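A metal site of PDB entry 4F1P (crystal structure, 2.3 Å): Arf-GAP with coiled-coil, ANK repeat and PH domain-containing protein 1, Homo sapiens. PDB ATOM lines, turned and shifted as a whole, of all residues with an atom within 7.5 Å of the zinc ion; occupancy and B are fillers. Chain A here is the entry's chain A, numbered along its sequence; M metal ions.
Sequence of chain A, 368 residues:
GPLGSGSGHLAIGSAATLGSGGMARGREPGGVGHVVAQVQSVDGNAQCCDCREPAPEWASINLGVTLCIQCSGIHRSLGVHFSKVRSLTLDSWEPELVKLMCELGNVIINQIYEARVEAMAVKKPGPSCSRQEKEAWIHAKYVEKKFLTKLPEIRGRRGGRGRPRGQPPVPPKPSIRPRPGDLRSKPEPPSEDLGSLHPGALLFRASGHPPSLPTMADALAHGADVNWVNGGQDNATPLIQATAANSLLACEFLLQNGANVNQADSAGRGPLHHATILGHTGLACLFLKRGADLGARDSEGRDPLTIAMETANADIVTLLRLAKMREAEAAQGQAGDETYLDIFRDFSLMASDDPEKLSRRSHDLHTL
The nearest printed residue that does not touch the zinc ion is Glu 53 (4.3 Å).
The side-chain sulfur (SG) of Cys 68 lies close to the backbone NH (N) of Gln 70 (3.8 Å). The backbone carbonyl oxygen of Cys 68 sits at hydrogen-bond distance from the side-chain hydroxyl of Ser 72, 3.3 Å away. N of Glu 53 sits close to SG of Cys 51 (3.4 Å). SG of Cys 51 sits close to NZ of Lys 134 (3.5 Å). The backbone carbonyl oxygen (O) of Glu 53 is in hydrogen-bond range of the backbone NH (N) of Cys 48 (2.6 Å). The side-chain sulfur (SG) of Cys 48 lies close to the backbone NH (N) of Asp 50 (3.4 Å).
The zinc ion is bound by SG of Cys 68, 2.2 Å away. The zinc ion is bound by the side-chain sulfur (SG) of Cys 71 (2.3 Å). SG of Cys 51 is bound to the zinc ion (2.4 Å). SG of Cys 48 is bound to the zinc ion (2.5 Å). The zinc ion has four donor atoms within binding distance.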
ATOM      1  N   GLN A  47     -29.620  29.731 -17.891  1.00  0.00           N
ATOM      2  CA  GLN A  47     -28.821  28.652 -17.313  1.00  0.00           C
ATOM      3  C   GLN A  47     -29.763  27.482 -17.015  1.00  0.00           C
ATOM      4  O   GLN A  47     -30.852  27.686 -16.476  1.00  0.00           O
ATOM      5  CB  GLN A  47     -28.182  29.105 -15.983  1.00  0.00           C
ATOM      6  CG  GLN A  47     -27.016  30.075 -16.108  1.00  0.00           C
ATOM      7  CD  GLN A  47     -27.458  31.480 -16.499  1.00  0.00           C
ATOM      8  OE1 GLN A  47     -28.354  32.051 -15.888  1.00  0.00           O
ATOM      9  NE2 GLN A  47     -26.816  32.027 -17.533  1.00  0.00           N
ATOM     10  N   CYS A  48     -29.362  26.262 -17.360  1.00  0.00           N
ATOM     11  CA  CYS A  48     -30.189  25.083 -17.065  1.00  0.00           C
ATOM     12  C   CYS A  48     -30.611  25.083 -15.598  1.00  0.00           C
ATOM     13  O   CYS A  48     -29.815  25.368 -14.711  1.00  0.00           O
ATOM     14  CB  CYS A  48     -29.453  23.788 -17.406  1.00  0.00           C
ATOM     15  SG  CYS A  48     -30.365  22.316 -16.899  1.00  0.00           S
ATOM     16  N   CYS A  49     -31.879  24.746 -15.360  1.00  0.00           N
ATOM     17  CA  CYS A  49     -32.444  24.728 -14.013  1.00  0.00           C
ATOM     18  C   CYS A  49     -31.683  23.776 -13.093  1.00  0.00           C
ATOM     19  O   CYS A  49     -31.586  24.029 -11.894  1.00  0.00           O
ATOM     20  CB  CYS A  49     -33.923  24.319 -14.054  1.00  0.00           C
ATOM     21  SG  CYS A  49     -34.810  24.522 -12.488  1.00  0.00           S
ATOM     22  N   ASP A  50     -31.135  22.700 -13.640  1.00  0.00           N
ATOM     23  CA  ASP A  50     -30.601  21.641 -12.794  1.00  0.00           C
ATOM     24  C   ASP A  50     -29.078  21.577 -12.671  1.00  0.00           C
ATOM     25  O   ASP A  50     -28.562  21.156 -11.641  1.00  0.00           O
ATOM     26  CB  ASP A  50     -31.182  20.284 -13.199  1.00  0.00           C
ATOM     27  CG  ASP A  50     -32.706  20.258 -13.119  1.00  0.00           C
ATOM     28  OD1 ASP A  50     -33.300  21.006 -12.308  1.00  0.00           O
ATOM     29  OD2 ASP A  50     -33.305  19.462 -13.862  1.00  0.00           O
ATOM     30  N   CYS A  51     -28.360  22.030 -13.709  1.00  0.00           N
ATOM     31  CA  CYS A  51     -26.902  21.962 -13.717  1.00  0.00           C
ATOM     32  C   CYS A  51     -26.262  23.274 -14.152  1.00  0.00           C
ATOM     33  O   CYS A  51     -25.036  23.417 -14.146  1.00  0.00           O
ATOM     34  CB  CYS A  51     -26.416  20.849 -14.631  1.00  0.00           C
ATOM     35  SG  CYS A  51     -26.465  21.282 -16.375  1.00  0.00           S
ATOM     36  N   ARG A  52     -27.110  24.217 -14.563  1.00  0.00           N
ATOM     37  CA  ARG A  52     -26.677  25.582 -14.933  1.00  0.00           C
ATOM     38  C   ARG A  52     -25.974  25.657 -16.273  1.00  0.00           C
ATOM     39  O   ARG A  52     -25.344  26.673 -16.574  1.00  0.00           O
ATOM     40  CB  ARG A  52     -25.853  26.245 -13.828  1.00  0.00           C
ATOM     41  CG  ARG A  52     -26.619  26.468 -12.531  1.00  0.00           C
ATOM     42  CD  ARG A  52     -25.822  27.317 -11.549  1.00  0.00           C
ATOM     43  NE  ARG A  52     -25.622  28.672 -12.038  1.00  0.00           N
ATOM     44  CZ  ARG A  52     -26.438  29.702 -11.787  1.00  0.00           C
ATOM     45  NH1 ARG A  52     -27.527  29.521 -11.068  1.00  0.00           N
ATOM     46  NH2 ARG A  52     -26.163  30.906 -12.286  1.00  0.00           N
ATOM     47  N   GLU A  53     -26.062  24.584 -17.067  1.00  0.00           N
ATOM     48  CA  GLU A  53     -25.571  24.583 -18.446  1.00  0.00           C
ATOM     49  C   GLU A  53     -26.154  25.786 -19.162  1.00  0.00           C
ATOM     50  O   GLU A  53     -27.360  26.041 -19.074  1.00  0.00           O
ATOM     51  CB  GLU A  53     -25.969  23.302 -19.174  1.00  0.00           C
ATOM     52  CG  GLU A  53     -25.564  23.221 -20.652  1.00  0.00           C
ATOM     53  CD  GLU A  53     -24.110  22.829 -20.861  1.00  0.00           C
ATOM     54  OE1 GLU A  53     -23.532  22.144 -19.997  1.00  0.00           O
ATOM     55  OE2 GLU A  53     -23.521  23.211 -21.919  1.00  0.00           O
ATOM     56  N   PRO A  54     -25.305  26.562 -19.854  1.00  0.00           N
ATOM     57  CA  PRO A  54     -25.758  27.763 -20.540  1.00  0.00           C
ATOM     58  C   PRO A  54     -26.681  27.489 -21.731  1.00  0.00           C
ATOM     59  O   PRO A  54     -26.631  26.408 -22.327  1.00  0.00           O
ATOM     60  CB  PRO A  54     -24.448  28.394 -21.043  1.00  0.00           C
ATOM     61  CG  PRO A  54     -23.369  27.771 -20.228  1.00  0.00           C
ATOM     62  CD  PRO A  54     -23.838  26.396 -19.933  1.00  0.00           C
ATOM     63  N   PRO A  56     -30.009  26.816 -22.315  1.00  0.00           N
ATOM     64  CA  PRO A  56     -30.832  25.590 -22.365  1.00  0.00           C
ATOM     65  C   PRO A  56     -31.979  25.726 -23.386  1.00  0.00           C
ATOM     66  O   PRO A  56     -32.691  26.725 -23.398  1.00  0.00           O
ATOM     67  CB  PRO A  56     -31.380  25.487 -20.949  1.00  0.00           C
ATOM     68  CG  PRO A  56     -31.459  26.898 -20.471  1.00  0.00           C
ATOM     69  CD  PRO A  56     -30.331  27.639 -21.132  1.00  0.00           C
ATOM     70  N   THR A  66     -36.484  25.736 -17.698  1.00  0.00           N
ATOM     71  CA  THR A  66     -35.647  25.450 -18.853  1.00  0.00           C
ATOM     72  C   THR A  66     -34.533  24.472 -18.479  1.00  0.00           C
ATOM     73  O   THR A  66     -33.964  24.542 -17.385  1.00  0.00           O
ATOM     74  CB  THR A  66     -35.034  26.729 -19.443  1.00  0.00           C
ATOM     75  OG1 THR A  66     -34.311  27.436 -18.424  1.00  0.00           O
ATOM     76  CG2 THR A  66     -36.120  27.628 -20.028  1.00  0.00           C
ATOM     77  N   LEU A  67     -34.261  23.551 -19.398  1.00  0.00           N
ATOM     78  CA  LEU A  67     -33.342  22.441 -19.181  1.00  0.00           C
ATOM     79  C   LEU A  67     -32.391  22.282 -20.366  1.00  0.00           C
ATOM     80  O   LEU A  67     -32.764  22.592 -21.510  1.00  0.00           O
ATOM     81  CB  LEU A  67     -34.114  21.134 -18.949  1.00  0.00           C
ATOM     82  CG  LEU A  67     -35.181  21.118 -17.848  1.00  0.00           C
ATOM     83  CD1 LEU A  67     -36.162  19.968 -18.073  1.00  0.00           C
ATOM     84  CD2 LEU A  67     -34.550  21.051 -16.458  1.00  0.00           C
ATOM     85  N   CYS A  68     -31.183  21.816 -20.091  1.00  0.00           N
ATOM     86  CA  CYS A  68     -30.203  21.516 -21.142  1.00  0.00           C
ATOM     87  C   CYS A  68     -30.515  20.154 -21.734  1.00  0.00           C
ATOM     88  O   CYS A  68     -31.334  19.414 -21.177  1.00  0.00           O
ATOM     89  CB  CYS A  68     -28.783  21.535 -20.563  1.00  0.00           C
ATOM     90  SG  CYS A  68     -28.445  20.258 -19.313  1.00  0.00           S
ATOM     91  N   ILE A  69     -29.874  19.814 -22.851  1.00  0.00           N
ATOM     92  CA  ILE A  69     -30.079  18.508 -23.508  1.00  0.00           C
ATOM     93  C   ILE A  69     -29.972  17.363 -22.489  1.00  0.00           C
ATOM     94  O   ILE A  69     -30.856  16.494 -22.423  1.00  0.00           O
ATOM     95  CB  ILE A  69     -29.115  18.286 -24.709  1.00  0.00           C
ATOM     96  CG1 ILE A  69     -29.407  19.303 -25.824  1.00  0.00           C
ATOM     97  CG2 ILE A  69     -29.237  16.872 -25.269  1.00  0.00           C
ATOM     98  CD1 ILE A  69     -28.329  19.411 -26.894  1.00  0.00           C
ATOM     99  N   GLN A  70     -28.918  17.378 -21.688  1.00  0.00           N
ATOM    100  CA  GLN A  70     -28.652  16.285 -20.752  1.00  0.00           C
ATOM    101  C   GLN A  70     -29.690  16.176 -19.630  1.00  0.00           C
ATOM    102  O   GLN A  70     -30.134  15.086 -19.292  1.00  0.00           O
ATOM    103  CB  GLN A  70     -27.244  16.393 -20.169  1.00  0.00           C
ATOM    104  CG  GLN A  70     -26.664  15.059 -19.726  1.00  0.00           C
ATOM    105  CD  GLN A  70     -25.244  15.196 -19.196  1.00  0.00           C
ATOM    106  OE1 GLN A  70     -24.805  16.294 -18.844  1.00  0.00           O
ATOM    107  NE2 GLN A  70     -24.542  14.081 -19.116  1.00  0.00           N
ATOM    108  N   CYS A  71     -30.072  17.307 -19.040  1.00  0.00           N
ATOM    109  CA  CYS A  71     -31.027  17.275 -17.958  1.00  0.00           C
ATOM    110  C   CYS A  71     -32.466  17.000 -18.452  1.00  0.00           C
ATOM    111  O   CYS A  71     -33.242  16.355 -17.741  1.00  0.00           O
ATOM    112  CB  CYS A  71     -30.929  18.541 -17.088  1.00  0.00           C
ATOM    113  SG  CYS A  71     -29.346  18.651 -16.181  1.00  0.00           S
ATOM    114  N   SER A  72     -32.790  17.459 -19.654  1.00  0.00           N
ATOM    115  CA  SER A  72     -34.097  17.149 -20.252  1.00  0.00           C
ATOM    116  C   SER A  72     -34.211  15.650 -20.496  1.00  0.00           C
ATOM    117  O   SER A  72     -35.271  15.055 -20.260  1.00  0.00           O
ATOM    118  CB  SER A  72     -34.328  17.920 -21.560  1.00  0.00           C
ATOM    119  OG  SER A  72     -33.511  17.434 -22.612  1.00  0.00           O
ATOM    120  N   ILE A  74     -32.788  13.303 -18.754  1.00  0.00           N
ATOM    121  CA  ILE A  74     -33.067  12.735 -17.437  1.00  0.00           C
ATOM    122  C   ILE A  74     -34.514  12.977 -16.998  1.00  0.00           C
ATOM    123  O   ILE A  74     -35.158  12.058 -16.496  1.00  0.00           O
ATOM    124  CB  ILE A  74     -32.064  13.252 -16.383  1.00  0.00           C
ATOM    125  CG1 ILE A  74     -30.628  12.893 -16.804  1.00  0.00           C
ATOM    126  CG2 ILE A  74     -32.379  12.657 -15.010  1.00  0.00           C
ATOM    127  CD1 ILE A  74     -29.540  13.756 -16.213  1.00  0.00           C
ATOM    128  N   PRO A 125     -24.804  20.091  -8.985  1.00  0.00           N
ATOM    129  CA  PRO A 125     -23.951  19.781 -10.124  1.00  0.00           C
ATOM    130  C   PRO A 125     -23.761  20.974 -11.050  1.00  0.00           C
ATOM    131  O   PRO A 125     -24.676  21.794 -11.201  1.00  0.00           O
ATOM    132  CB  PRO A 125     -24.719  18.654 -10.844  1.00  0.00           C
ATOM    133  CG  PRO A 125     -26.125  18.795 -10.382  1.00  0.00           C
ATOM    134  CD  PRO A 125     -26.006  19.235  -8.954  1.00  0.00           C
ATOM    135  N   GLY A 126     -22.570  21.074 -11.629  1.00  0.00           N
ATOM    136  CA  GLY A 126     -22.291  22.040 -12.690  1.00  0.00           C
ATOM    137  C   GLY A 126     -22.465  21.435 -14.079  1.00  0.00           C
ATOM    138  O   GLY A 126     -22.804  20.250 -14.204  1.00  0.00           O
ATOM    139  N   PRO A 127     -22.228  22.234 -15.134  1.00  0.00           N
ATOM    140  CA  PRO A 127     -22.389  21.802 -16.535  1.00  0.00           C
ATOM    141  C   PRO A 127     -21.570  20.566 -16.888  1.00  0.00           C
ATOM    142  O   PRO A 127     -22.045  19.709 -17.645  1.00  0.00           O
ATOM    143  CB  PRO A 127     -21.865  23.010 -17.318  1.00  0.00           C
ATOM    144  CG  PRO A 127     -22.134  24.175 -16.430  1.00  0.00           C
ATOM    145  CD  PRO A 127     -21.842  23.661 -15.051  1.00  0.00           C
ATOM    146  N   LYS A 134     -25.837  14.189 -12.224  1.00  0.00           N
ATOM    147  CA  LYS A 134     -27.027  14.935 -12.582  1.00  0.00           C
ATOM    148  C   LYS A 134     -28.311  14.118 -12.334  1.00  0.00           C
ATOM    149  O   LYS A 134     -29.267  14.663 -11.819  1.00  0.00           O
ATOM    150  CB  LYS A 134     -26.956  15.467 -14.023  1.00  0.00           C
ATOM    151  CG  LYS A 134     -25.820  16.448 -14.277  1.00  0.00           C
ATOM    152  CD  LYS A 134     -25.926  17.107 -15.639  1.00  0.00           C
ATOM    153  CE  LYS A 134     -24.722  17.985 -15.937  1.00  0.00           C
ATOM    154  NZ  LYS A 134     -24.686  18.471 -17.345  1.00  0.00           N
ATOM    155  N   ILE A 138     -31.287  15.355  -9.861  1.00  0.00           N
ATOM    156  CA  ILE A 138     -32.619  15.566 -10.424  1.00  0.00           C
ATOM    157  C   ILE A 138     -33.660  14.712  -9.709  1.00  0.00           C
ATOM    158  O   ILE A 138     -34.730  15.195  -9.355  1.00  0.00           O
ATOM    159  CB  ILE A 138     -32.617  15.349 -11.960  1.00  0.00           C
ATOM    160  CG1 ILE A 138     -31.876  16.530 -12.623  1.00  0.00           C
ATOM    161  CG2 ILE A 138     -34.037  15.217 -12.512  1.00  0.00           C
ATOM    162  CD1 ILE A 138     -31.490  16.285 -14.067  1.00  0.00           C
HETATM  163 ZN    ZN M   1     -28.622  20.595 -17.123  1.00  0.00          ZN
